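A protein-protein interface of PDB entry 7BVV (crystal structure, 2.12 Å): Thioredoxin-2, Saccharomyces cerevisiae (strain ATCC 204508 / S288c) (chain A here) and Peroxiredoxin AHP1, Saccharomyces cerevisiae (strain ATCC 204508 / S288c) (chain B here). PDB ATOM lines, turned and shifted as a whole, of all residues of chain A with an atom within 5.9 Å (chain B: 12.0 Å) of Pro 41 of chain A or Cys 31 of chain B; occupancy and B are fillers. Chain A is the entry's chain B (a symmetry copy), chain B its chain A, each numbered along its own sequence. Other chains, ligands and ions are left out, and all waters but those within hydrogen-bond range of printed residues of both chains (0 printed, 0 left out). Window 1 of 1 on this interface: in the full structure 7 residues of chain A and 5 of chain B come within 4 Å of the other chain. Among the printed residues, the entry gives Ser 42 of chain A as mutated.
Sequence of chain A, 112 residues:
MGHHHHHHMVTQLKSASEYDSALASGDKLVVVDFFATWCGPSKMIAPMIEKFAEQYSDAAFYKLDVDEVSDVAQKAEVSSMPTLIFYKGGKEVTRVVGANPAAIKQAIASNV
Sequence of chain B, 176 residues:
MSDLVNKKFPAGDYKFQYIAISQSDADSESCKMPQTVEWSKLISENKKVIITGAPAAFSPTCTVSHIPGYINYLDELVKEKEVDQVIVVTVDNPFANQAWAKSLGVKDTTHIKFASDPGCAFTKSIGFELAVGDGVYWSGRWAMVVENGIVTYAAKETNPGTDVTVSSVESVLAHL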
ATOM      1  N   ALA A  36      28.446  35.904 -20.704  1.00  0.00           N
ATOM      2  CA  ALA A  36      29.456  35.353 -21.623  1.00  0.00           C
ATOM      3  C   ALA A  36      29.044  35.708 -23.037  1.00  0.00           C
ATOM      4  O   ALA A  36      27.812  35.744 -23.291  1.00  0.00           O
ATOM      5  CB  ALA A  36      29.550  33.862 -21.418  1.00  0.00           C
ATOM      6  N   TRP A  38      29.445  34.063 -25.794  1.00  0.00           N
ATOM      7  CA  TRP A  38      28.934  32.863 -26.507  1.00  0.00           C
ATOM      8  C   TRP A  38      27.538  32.466 -26.005  1.00  0.00           C
ATOM      9  O   TRP A  38      27.006  31.523 -26.536  1.00  0.00           O
ATOM     10  CB  TRP A  38      29.931  31.718 -26.321  1.00  0.00           C
ATOM     11  CG  TRP A  38      30.345  31.498 -24.898  1.00  0.00           C
ATOM     12  CD1 TRP A  38      31.471  31.966 -24.285  1.00  0.00           C
ATOM     13  CD2 TRP A  38      29.614  30.775 -23.888  1.00  0.00           C
ATOM     14  NE1 TRP A  38      31.501  31.562 -22.977  1.00  0.00           N
ATOM     15  CE2 TRP A  38      30.400  30.802 -22.712  1.00  0.00           C
ATOM     16  CE3 TRP A  38      28.409  30.058 -23.882  1.00  0.00           C
ATOM     17  CZ2 TRP A  38      30.007  30.171 -21.532  1.00  0.00           C
ATOM     18  CZ3 TRP A  38      28.035  29.397 -22.728  1.00  0.00           C
ATOM     19  CH2 TRP A  38      28.820  29.462 -21.570  1.00  0.00           C
ATOM     20  N   CYS A  39      26.990  33.138 -24.990  1.00  0.00           N
ATOM     21  CA  CYS A  39      25.806  32.684 -24.218  1.00  0.00           C
ATOM     22  C   CYS A  39      24.545  33.404 -24.709  1.00  0.00           C
ATOM     23  O   CYS A  39      24.418  34.655 -24.528  1.00  0.00           O
ATOM     24  CB  CYS A  39      26.004  32.951 -22.731  1.00  0.00           C
ATOM     25  SG  CYS A  39      24.568  32.499 -21.723  1.00  0.00           S
ATOM     26  N   GLY A  40      23.646  32.652 -25.341  1.00  0.00           N
ATOM     27  CA  GLY A  40      22.376  33.182 -25.887  1.00  0.00           C
ATOM     28  C   GLY A  40      21.543  33.903 -24.826  1.00  0.00           C
ATOM     29  O   GLY A  40      21.157  35.057 -24.984  1.00  0.00           O
ATOM     30  N   PRO A  41      21.207  33.239 -23.709  1.00  0.00           N
ATOM     31  CA  PRO A  41      20.516  33.915 -22.612  1.00  0.00           C
ATOM     32  C   PRO A  41      21.161  35.238 -22.157  1.00  0.00           C
ATOM     33  O   PRO A  41      20.415  36.153 -21.816  1.00  0.00           O
ATOM     34  CB  PRO A  41      20.559  32.871 -21.499  1.00  0.00           C
ATOM     35  CG  PRO A  41      20.610  31.534 -22.227  1.00  0.00           C
ATOM     36  CD  PRO A  41      21.420  31.809 -23.470  1.00  0.00           C
ATOM     37  N   SER A  42      22.502  35.337 -22.188  1.00  0.00           N
ATOM     38  CA  SER A  42      23.225  36.592 -21.848  1.00  0.00           C
ATOM     39  C   SER A  42      22.757  37.678 -22.818  1.00  0.00           C
ATOM     40  O   SER A  42      22.343  38.767 -22.373  1.00  0.00           O
ATOM     41  CB  SER A  42      24.738  36.430 -21.854  1.00  0.00           C
ATOM     42  OG  SER A  42      25.160  35.669 -20.729  1.00  0.00           O
ATOM     43  N   LYS A  43      22.817  37.368 -24.105  1.00  0.00           N
ATOM     44  CA  LYS A  43      22.538  38.345 -25.175  1.00  0.00           C
ATOM     45  C   LYS A  43      21.058  38.766 -25.103  1.00  0.00           C
ATOM     46  O   LYS A  43      20.752  39.918 -25.476  1.00  0.00           O
ATOM     47  CB  LYS A  43      22.958  37.749 -26.518  1.00  0.00           C
ATOM     48  CG  LYS A  43      24.462  37.756 -26.762  1.00  0.00           C
ATOM     49  CD  LYS A  43      24.966  36.678 -27.708  1.00  0.00           C
ATOM     50  CE  LYS A  43      24.959  37.129 -29.151  1.00  0.00           C
ATOM     51  NZ  LYS A  43      24.876  35.982 -30.085  1.00  0.00           N
ATOM     52  N   MET A  44      20.194  37.931 -24.534  1.00  0.00           N
ATOM     53  CA  MET A  44      18.733  38.202 -24.462  1.00  0.00           C
ATOM     54  C   MET A  44      18.414  39.089 -23.265  1.00  0.00           C
ATOM     55  O   MET A  44      17.550  39.947 -23.424  1.00  0.00           O
ATOM     56  CB  MET A  44      17.918  36.913 -24.320  1.00  0.00           C
ATOM     57  CG  MET A  44      17.892  36.066 -25.568  1.00  0.00           C
ATOM     58  SD  MET A  44      16.618  34.795 -25.463  1.00  0.00           S
ATOM     59  CE  MET A  44      16.981  33.956 -23.921  1.00  0.00           C
ATOM     60  N   ILE A  45      19.064  38.856 -22.119  1.00  0.00           N
ATOM     61  CA  ILE A  45      18.781  39.610 -20.871  1.00  0.00           C
ATOM     62  C   ILE A  45      19.394  41.011 -21.005  1.00  0.00           C
ATOM     63  O   ILE A  45      18.928  41.934 -20.314  1.00  0.00           O
ATOM     64  CB  ILE A  45      19.232  38.850 -19.612  1.00  0.00           C
ATOM     65  CG1 ILE A  45      18.493  39.363 -18.367  1.00  0.00           C
ATOM     66  CG2 ILE A  45      20.745  38.909 -19.405  1.00  0.00           C
ATOM     67  CD1 ILE A  45      16.988  39.112 -18.362  1.00  0.00           C
ATOM     68  N   ALA A  46      20.379  41.192 -21.879  1.00  0.00           N
ATOM     69  CA  ALA A  46      21.199  42.427 -21.899  1.00  0.00           C
ATOM     70  C   ALA A  46      20.332  43.679 -22.101  1.00  0.00           C
ATOM     71  O   ALA A  46      20.425  44.612 -21.305  1.00  0.00           O
ATOM     72  CB  ALA A  46      22.292  42.288 -22.918  1.00  0.00           C
ATOM     73  N   SER A  79      28.500  29.878 -11.717  1.00  0.00           N
ATOM     74  CA  SER A  79      28.628  28.591 -12.444  1.00  0.00           C
ATOM     75  C   SER A  79      27.650  28.557 -13.619  1.00  0.00           C
ATOM     76  O   SER A  79      27.655  27.589 -14.380  1.00  0.00           O
ATOM     77  CB  SER A  79      28.372  27.465 -11.511  1.00  0.00           C
ATOM     78  OG  SER A  79      27.074  27.597 -10.945  1.00  0.00           O
ATOM     79  N   SER A  80      26.828  29.586 -13.752  1.00  0.00           N
ATOM     80  CA  SER A  80      25.761  29.667 -14.774  1.00  0.00           C
ATOM     81  C   SER A  80      25.612  31.135 -15.159  1.00  0.00           C
ATOM     82  O   SER A  80      25.821  31.975 -14.288  1.00  0.00           O
ATOM     83  CB  SER A  80      24.459  29.084 -14.279  1.00  0.00           C
ATOM     84  OG  SER A  80      23.602  28.849 -15.363  1.00  0.00           O
ATOM     85  N   MET A  81      25.301  31.404 -16.428  1.00  0.00           N
ATOM     86  CA  MET A  81      25.078  32.755 -16.980  1.00  0.00           C
ATOM     87  C   MET A  81      23.704  32.747 -17.645  1.00  0.00           C
ATOM     88  O   MET A  81      23.348  31.799 -18.346  1.00  0.00           O
ATOM     89  CB  MET A  81      26.140  33.133 -18.018  1.00  0.00           C
ATOM     90  CG  MET A  81      27.486  33.557 -17.442  1.00  0.00           C
ATOM     91  SD  MET A  81      28.368  32.177 -16.681  1.00  0.00           S
ATOM     92  CE  MET A  81      28.795  31.240 -18.145  1.00  0.00           C
ATOM     93  N   PRO A  82      22.891  33.811 -17.482  1.00  0.00           N
ATOM     94  CA  PRO A  82      23.221  34.962 -16.644  1.00  0.00           C
ATOM     95  C   PRO A  82      23.166  34.671 -15.143  1.00  0.00           C
ATOM     96  O   PRO A  82      22.382  33.846 -14.684  1.00  0.00           O
ATOM     97  CB  PRO A  82      22.139  36.008 -16.962  1.00  0.00           C
ATOM     98  CG  PRO A  82      21.495  35.499 -18.245  1.00  0.00           C
ATOM     99  CD  PRO A  82      21.605  33.995 -18.159  1.00  0.00           C
ATOM    100  N   ALA A  99      17.949  33.879 -17.269  1.00  0.00           N
ATOM    101  CA  ALA A  99      17.307  34.984 -18.005  1.00  0.00           C
ATOM    102  C   ALA A  99      15.854  35.097 -17.529  1.00  0.00           C
ATOM    103  O   ALA A  99      14.945  34.711 -18.269  1.00  0.00           O
ATOM    104  CB  ALA A  99      17.409  34.756 -19.501  1.00  0.00           C
ATOM    105  N   TYR B  18      33.772  19.696 -12.681  1.00  0.00           N
ATOM    106  CA  TYR B  18      32.608  19.158 -13.423  1.00  0.00           C
ATOM    107  C   TYR B  18      31.671  20.297 -13.800  1.00  0.00           C
ATOM    108  O   TYR B  18      31.762  21.399 -13.215  1.00  0.00           O
ATOM    109  CB  TYR B  18      31.849  18.126 -12.604  1.00  0.00           C
ATOM    110  CG  TYR B  18      30.852  18.703 -11.635  1.00  0.00           C
ATOM    111  CD1 TYR B  18      31.260  19.319 -10.465  1.00  0.00           C
ATOM    112  CD2 TYR B  18      29.490  18.551 -11.846  1.00  0.00           C
ATOM    113  CE1 TYR B  18      30.353  19.871  -9.577  1.00  0.00           C
ATOM    114  CE2 TYR B  18      28.564  19.104 -10.976  1.00  0.00           C
ATOM    115  CZ  TYR B  18      29.003  19.761  -9.842  1.00  0.00           C
ATOM    116  OH  TYR B  18      28.104  20.281  -8.973  1.00  0.00           O
ATOM    117  N   ILE B  19      30.824  20.040 -14.785  1.00  0.00           N
ATOM    118  CA  ILE B  19      29.767  21.006 -15.194  1.00  0.00           C
ATOM    119  C   ILE B  19      28.413  20.398 -14.855  1.00  0.00           C
ATOM    120  O   ILE B  19      28.176  19.213 -15.187  1.00  0.00           O
ATOM    121  CB  ILE B  19      29.881  21.370 -16.681  1.00  0.00           C
ATOM    122  CG1 ILE B  19      31.301  21.826 -17.035  1.00  0.00           C
ATOM    123  CG2 ILE B  19      28.817  22.415 -17.030  1.00  0.00           C
ATOM    124  CD1 ILE B  19      31.489  22.251 -18.474  1.00  0.00           C
ATOM    125  N   ALA B  20      27.575  21.175 -14.173  1.00  0.00           N
ATOM    126  CA  ALA B  20      26.253  20.722 -13.685  1.00  0.00           C
ATOM    127  C   ALA B  20      25.329  20.503 -14.879  1.00  0.00           C
ATOM    128  O   ALA B  20      25.552  21.103 -15.949  1.00  0.00           O
ATOM    129  CB  ALA B  20      25.662  21.708 -12.725  1.00  0.00           C
ATOM    130  N   ILE B  21      24.357  19.621 -14.703  1.00  0.00           N
ATOM    131  CA  ILE B  21      23.245  19.414 -15.661  1.00  0.00           C
ATOM    132  C   ILE B  21      22.002  19.423 -14.793  1.00  0.00           C
ATOM    133  O   ILE B  21      22.080  18.856 -13.689  1.00  0.00           O
ATOM    134  CB  ILE B  21      23.376  18.090 -16.435  1.00  0.00           C
ATOM    135  CG1 ILE B  21      24.726  17.941 -17.135  1.00  0.00           C
ATOM    136  CG2 ILE B  21      22.221  17.930 -17.422  1.00  0.00           C
ATOM    137  CD1 ILE B  21      24.974  16.551 -17.666  1.00  0.00           C
ATOM    138  N   SER B  22      20.952  20.105 -15.237  1.00  0.00           N
ATOM    139  CA  SER B  22      19.628  20.135 -14.562  1.00  0.00           C
ATOM    140  C   SER B  22      18.538  19.797 -15.580  1.00  0.00           C
ATOM    141  O   SER B  22      18.806  19.877 -16.808  1.00  0.00           O
ATOM    142  CB  SER B  22      19.361  21.465 -13.911  1.00  0.00           C
ATOM    143  OG  SER B  22      19.411  22.504 -14.875  1.00  0.00           O
ATOM    144  N   GLN B  23      17.361  19.411 -15.079  1.00  0.00           N
ATOM    145  CA  GLN B  23      16.206  18.991 -15.927  1.00  0.00           C
ATOM    146  C   GLN B  23      15.818  20.122 -16.904  1.00  0.00           C
ATOM    147  O   GLN B  23      15.505  19.778 -18.047  1.00  0.00           O
ATOM    148  CB  GLN B  23      15.032  18.521 -15.059  1.00  0.00           C
ATOM    149  CG  GLN B  23      15.277  17.190 -14.337  1.00  0.00           C
ATOM    150  CD  GLN B  23      15.267  15.955 -15.221  1.00  0.00           C
ATOM    151  OE1 GLN B  23      14.751  15.934 -16.342  1.00  0.00           O
ATOM    152  NE2 GLN B  23      15.842  14.881 -14.713  1.00  0.00           N
ATOM    153  N   SER B  24      15.927  21.402 -16.504  1.00  0.00           N
ATOM    154  CA  SER B  24      15.726  22.619 -17.351  1.00  0.00           C
ATOM    155  C   SER B  24      16.497  22.538 -18.685  1.00  0.00           C
ATOM    156  O   SER B  24      15.985  23.062 -19.688  1.00  0.00           O
ATOM    157  CB  SER B  24      16.131  23.872 -16.615  1.00  0.00           C
ATOM    158  OG  SER B  24      15.463  23.979 -15.375  1.00  0.00           O
ATOM    159  N   ASP B  25      17.677  21.910 -18.681  1.00  0.00           N
ATOM    160  CA  ASP B  25      18.538  21.743 -19.883  1.00  0.00           C
ATOM    161  C   ASP B  25      17.947  20.667 -20.809  1.00  0.00           C
ATOM    162  O   ASP B  25      17.104  19.890 -20.348  1.00  0.00           O
ATOM    163  CB  ASP B  25      19.975  21.382 -19.500  1.00  0.00           C
ATOM    164  CG  ASP B  25      20.594  22.214 -18.390  1.00  0.00           C
ATOM    165  OD1 ASP B  25      20.225  23.378 -18.227  1.00  0.00           O
ATOM    166  OD2 ASP B  25      21.420  21.680 -17.704  1.00  0.00           O
ATOM    167  N   ALA B  26      18.429  20.626 -22.061  1.00  0.00           N
ATOM    168  CA  ALA B  26      17.954  19.715 -23.134  1.00  0.00           C
ATOM    169  C   ALA B  26      16.467  19.981 -23.407  1.00  0.00           C
ATOM    170  O   ALA B  26      15.814  19.148 -24.066  1.00  0.00           O
ATOM    171  CB  ALA B  26      18.262  18.260 -22.847  1.00  0.00           C
ATOM    172  N   ASP B  27      15.976  21.117 -22.900  1.00  0.00           N
ATOM    173  CA  ASP B  27      14.584  21.610 -23.082  1.00  0.00           C
ATOM    174  C   ASP B  27      14.697  23.116 -23.341  1.00  0.00           C
ATOM    175  O   ASP B  27      14.003  23.632 -24.240  1.00  0.00           O
ATOM    176  CB  ASP B  27      13.713  21.296 -21.864  1.00  0.00           C
ATOM    177  CG  ASP B  27      12.447  22.132 -21.797  1.00  0.00           C
ATOM    178  OD1 ASP B  27      11.540  21.887 -22.618  1.00  0.00           O
ATOM    179  OD2 ASP B  27      12.376  23.021 -20.927  1.00  0.00           O
ATOM    180  N   SER B  28      15.560  23.768 -22.556  1.00  0.00           N
ATOM    181  CA  SER B  28      15.908  25.207 -22.670  1.00  0.00           C
ATOM    182  C   SER B  28      17.391  25.374 -23.015  1.00  0.00           C
ATOM    183  O   SER B  28      18.119  24.361 -23.042  1.00  0.00           O
ATOM    184  CB  SER B  28      15.556  25.929 -21.406  1.00  0.00           C
ATOM    185  OG  SER B  28      14.207  25.668 -21.069  1.00  0.00           O
ATOM    186  N   GLU B  29      17.808  26.604 -23.310  1.00  0.00           N
ATOM    187  CA  GLU B  29      19.233  26.929 -23.549  1.00  0.00           C
ATOM    188  C   GLU B  29      19.855  27.360 -22.223  1.00  0.00           C
ATOM    189  O   GLU B  29      19.247  28.174 -21.513  1.00  0.00           O
ATOM    190  CB  GLU B  29      19.388  28.033 -24.588  1.00  0.00           C
ATOM    191  CG  GLU B  29      20.823  28.227 -25.057  1.00  0.00           C
ATOM    192  CD  GLU B  29      20.946  29.152 -26.260  1.00  0.00           C
ATOM    193  OE1 GLU B  29      21.952  29.906 -26.337  1.00  0.00           O
ATOM    194  OE2 GLU B  29      20.024  29.108 -27.137  1.00  0.00           O
ATOM    195  N   SER B  30      21.012  26.800 -21.900  1.00  0.00           N
ATOM    196  CA  SER B  30      21.729  27.050 -20.624  1.00  0.00           C
ATOM    197  C   SER B  30      23.191  27.370 -20.941  1.00  0.00           C
ATOM    198  O   SER B  30      23.663  27.058 -22.066  1.00  0.00           O
ATOM    199  CB  SER B  30      21.603  25.896 -19.648  1.00  0.00           C
ATOM    200  OG  SER B  30      22.553  24.872 -19.929  1.00  0.00           O
ATOM    201  N   CYS B  31      23.859  27.999 -19.982  1.00  0.00           N
ATOM    202  CA  CYS B  31      25.265  28.448 -20.089  1.00  0.00           C
ATOM    203  C   CYS B  31      25.958  28.123 -18.777  1.00  0.00           C
ATOM    204  O   CYS B  31      26.090  28.997 -17.913  1.00  0.00           O
ATOM    205  CB  CYS B  31      25.311  29.925 -20.428  1.00  0.00           C
ATOM    206  SG  CYS B  31      24.421  30.327 -21.951  1.00  0.00           S
ATOM    207  N   LYS B  32      26.304  26.861 -18.614  1.00  0.00           N
ATOM    208  CA  LYS B  32      26.939  26.351 -17.390  1.00  0.00           C
ATOM    209  C   LYS B  32      28.452  26.403 -17.579  1.00  0.00           C
ATOM    210  O   LYS B  32      28.912  26.246 -18.689  1.00  0.00           O
ATOM    211  CB  LYS B  32      26.417  24.947 -17.079  1.00  0.00           C
ATOM    212  CG  LYS B  32      25.421  24.891 -15.936  1.00  0.00           C
ATOM    213  CD  LYS B  32      24.005  25.045 -16.379  1.00  0.00           C
ATOM    214  CE  LYS B  32      23.024  24.636 -15.305  1.00  0.00           C
ATOM    215  NZ  LYS B  32      21.682  24.430 -15.884  1.00  0.00           N
ATOM    216  N   MET B  33      29.172  26.641 -16.496  1.00  0.00           N
ATOM    217  CA  MET B  33      30.647  26.724 -16.446  1.00  0.00           C
ATOM    218  C   MET B  33      31.159  25.639 -15.487  1.00  0.00           C
ATOM    219  O   MET B  33      30.412  25.135 -14.656  1.00  0.00           O
ATOM    220  CB  MET B  33      31.074  28.132 -15.996  1.00  0.00           C
ATOM    221  CG  MET B  33      32.189  28.751 -16.850  1.00  0.00           C
ATOM    222  SD  MET B  33      31.897  28.694 -18.663  1.00  0.00           S
ATOM    223  CE  MET B  33      33.547  28.450 -19.318  1.00  0.00           C
ATOM    224  N   PRO B  34      32.426  25.181 -15.653  1.00  0.00           N
ATOM    225  CA  PRO B  34      33.074  24.295 -14.699  1.00  0.00           C
ATOM    226  C   PRO B  34      33.014  24.810 -13.257  1.00  0.00           C
ATOM    227  O   PRO B  34      33.155  25.951 -13.051  1.00  0.00           O
ATOM    228  CB  PRO B  34      34.534  24.267 -15.168  1.00  0.00           C
ATOM    229  CG  PRO B  34      34.475  24.540 -16.615  1.00  0.00           C
ATOM    230  CD  PRO B  34      33.291  25.450 -16.810  1.00  0.00           C
ATOM    231  N   GLN B  35      32.805  23.901 -12.320  1.00  0.00           N
ATOM    232  CA  GLN B  35      32.901  24.111 -10.869  1.00  0.00           C
ATOM    233  C   GLN B  35      34.033  23.242 -10.337  1.00  0.00           C
ATOM    234  O   GLN B  35      34.141  22.084 -10.778  1.00  0.00           O
ATOM    235  CB  GLN B  35      31.618  23.646 -10.199  1.00  0.00           C
ATOM    236  CG  GLN B  35      30.397  24.429 -10.623  1.00  0.00           C
ATOM    237  CD  GLN B  35      29.188  23.915  -9.883  1.00  0.00           C
ATOM    238  OE1 GLN B  35      29.197  23.813  -8.660  1.00  0.00           O
ATOM    239  NE2 GLN B  35      28.145  23.606 -10.636  1.00  0.00           N
ATOM    240  N   PRO B  94      36.343  19.324 -18.751  1.00  0.00           N
ATOM    241  CA  PRO B  94      35.016  19.188 -18.159  1.00  0.00           C
ATOM    242  C   PRO B  94      33.884  19.396 -19.164  1.00  0.00           C
ATOM    243  O   PRO B  94      32.837  18.866 -18.948  1.00  0.00           O
ATOM    244  CB  PRO B  94      34.992  20.252 -17.073  1.00  0.00           C
ATOM    245  CG  PRO B  94      36.061  21.258 -17.501  1.00  0.00           C
ATOM    246  CD  PRO B  94      37.132  20.416 -18.153  1.00  0.00           C
ATOM    247  N   PHE B  95      34.140  20.138 -20.243  1.00  0.00           N
ATOM    248  CA  PHE B  95      33.131  20.390 -21.303  1.00  0.00           C
ATOM    249  C   PHE B  95      32.913  19.095 -22.066  1.00  0.00           C
ATOM    250  O   PHE B  95      31.754  18.771 -22.379  1.00  0.00           O
ATOM    251  CB  PHE B  95      33.517  21.533 -22.243  1.00  0.00           C
ATOM    252  CG  PHE B  95      33.926  22.802 -21.542  1.00  0.00           C
ATOM    253  CD1 PHE B  95      32.965  23.679 -21.055  1.00  0.00           C
ATOM    254  CD2 PHE B  95      35.268  23.115 -21.373  1.00  0.00           C
ATOM    255  CE1 PHE B  95      33.341  24.848 -20.412  1.00  0.00           C
ATOM    256  CE2 PHE B  95      35.641  24.273 -20.701  1.00  0.00           C
ATOM    257  CZ  PHE B  95      34.676  25.143 -20.235  1.00  0.00           C
ATOM    258  N   GLN B  98      31.009  16.636 -19.855  1.00  0.00           N
ATOM    259  CA  GLN B  98      29.585  17.032 -19.744  1.00  0.00           C
ATOM    260  C   GLN B  98      28.833  16.632 -21.008  1.00  0.00           C
ATOM    261  O   GLN B  98      27.677  16.103 -20.913  1.00  0.00           O
ATOM    262  CB  GLN B  98      29.421  18.535 -19.507  1.00  0.00           C
ATOM    263  CG  GLN B  98      27.999  18.907 -19.072  1.00  0.00           C
ATOM    264  CD  GLN B  98      27.497  20.199 -19.658  1.00  0.00           C
ATOM    265  OE1 GLN B  98      27.925  20.604 -20.719  1.00  0.00           O
ATOM    266  NE2 GLN B  98      26.592  20.858 -18.957  1.00  0.00           N
ATOM    267  N   LYS B 102      25.677  13.892 -21.339  1.00  0.00           N
ATOM    268  CA  LYS B 102      24.396  14.226 -22.021  1.00  0.00           C
ATOM    269  C   LYS B 102      24.155  13.243 -23.171  1.00  0.00           C
ATOM    270  O   LYS B 102      23.004  12.792 -23.334  1.00  0.00           O
ATOM    271  CB  LYS B 102      24.416  15.643 -22.570  1.00  0.00           C
ATOM    272  CG  LYS B 102      24.407  16.736 -21.514  1.00  0.00           C
ATOM    273  CD  LYS B 102      24.411  18.109 -22.168  1.00  0.00           C
ATOM    274  CE  LYS B 102      24.116  19.224 -21.183  1.00  0.00           C
ATOM    275  NZ  LYS B 102      24.329  20.564 -21.789  1.00  0.00           N
ATOM    276  N   THR B 109      22.691  16.247 -12.704  1.00  0.00           N
ATOM    277  CA  THR B 109      23.962  15.920 -11.991  1.00  0.00           C
ATOM    278  C   THR B 109      23.832  15.944 -10.461  1.00  0.00           C
ATOM    279  O   THR B 109      24.876  15.936  -9.796  1.00  0.00           O
ATOM    280  CB  THR B 109      25.102  16.830 -12.442  1.00  0.00           C
ATOM    281  OG1 THR B 109      24.658  18.182 -12.374  1.00  0.00           O
ATOM    282  CG2 THR B 109      25.565  16.498 -13.844  1.00  0.00           C
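No residue of chain B comes within 4 Å of Ala 36 of chain A.
Of chain B, only Cys 31 (3.6 Å) and Met 33 (3.7 Å) come within 4 Å of Trp 38 of chain A.
Of chain B, only Cys 31 comes within 4 Å of Cys 39 of chain A.
Of chain B, only Glu 29 (3.3 Å) comes within 4 Å of Gly 40 of chain A.
Pro 41 of chain A touches just these residues of chain B: Glu 29 (3.5 Å) and Cys 31 (3.7 Å).
No residue of chain B comes within 4 Å of Ser 42 of chain A.
No residue of chain B comes within 4 Å of Lys 43 of chain A.
No residue of chain B comes within 4 Å of Ile 45 of chain A.
Of chain B, only Lys 32 (3.3 Å), Met 33 (2.8 Å) and Gln 35 (3.8 Å) come within 4 Å of Ser 79 of chain A.
No residue of chain B comes within 4 Å of Pro 82 of chain A.
No residue of chain B comes within 4 Å of Ala 99 of chain A.
Ser 28 of chain B touches none of the printed residues of chain A.
Of the printed residues of chain A, Glu 29 of chain B touches Gly 40 and Pro 41.
Cys 31 of chain B touches just these residues of chain A: Trp 38 (3.6 Å), Cys 39 (2.2 Å), Pro 41 (3.7 Å), Ser 80 (3.2 Å) and Met 81 (2.9 Å).
Of the printed residues of chain A, Lys 32 of chain B touches Ser 79 and Ser 80.
Of the printed residues of chain A, Met 33 of chain B touches Trp 38 (3.7 Å) and Ser 79 (2.8 Å).
Of the printed residues of chain A, Gln 35 of chain B touches Ser 79 (3.8 Å).
Lys 102 of chain B touches none of the printed residues of chain A.
The nearest residue of chain B that does not touch Pro 41 of chain A is Ser 30 of chain B (4.8 Å).
The nearest residue of chain A that does not touch Cys 31 of chain B is Ser 79 of chain A (4.1 Å).
Among the printed residues, merely in contact across the chains: Ser 80 of chain A with Cys 31 of chain B, Ser 79 of chain A with Lys 32 of chain B, Pro 41 of chain A with Glu 29 of chain B, Trp 38 of chain A with Cys 31 of chain B, Pro 41 of chain A with Cys 31 of chain B, Trp 38 of chain A with Met 33 of chain B, Ser 79 of chain A with Gln 35 of chain B and Ser 80 of chain A with Lys 32 of chain B.
The backbone NH (N) of Gly 40 of chain A sits close to the side-chain carboxylate (OE1) of Glu 29 of chain B (3.4 Å).
SG of Cys 31 of chain B forms a disulfide with SG of Cys 39 of chain A (2.2 Å).
The backbone NH of Met 81 of chain A lies within hydrogen-bond range of the backbone carbonyl oxygen of Cys 31 of chain B, at 2.9 Å.
The backbone NH (N) of Met 33 of chain B is in hydrogen-bond range of the backbone carbonyl oxygen (O) of Ser 79 of chain A, 2.8 Å away.
Printed residues of chain B that touch a printed residue of chain A: Glu 29, Cys 31, Lys 32, Met 33 and Gln 35.
Along chain B the printed residues that touch a printed residue of chain A span positions 29 to 35.
Among the printed residues, 12 pairs touch across the chains.
O of Tyr 18 of chain B lies within hydrogen-bond range of N of Gln 35 of chain B, 2.9 Å away.
The side-chain hydroxyl (OG) of Ser 22 of chain B lies within hydrogen-bond range of the side-chain amino group (NZ) of Lys 32 of chain B, at 3.1 Å.
NZ of Lys 32 of chain B lies within salt-bridge range of OD1 of Asp 25 of chain B.
The side-chain sulfur (SG) of Cys 39 of chain A sits at hydrogen-bond distance from the side-chain hydroxyl (OG) of Ser 42 of chain A, 3.4 Å away.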
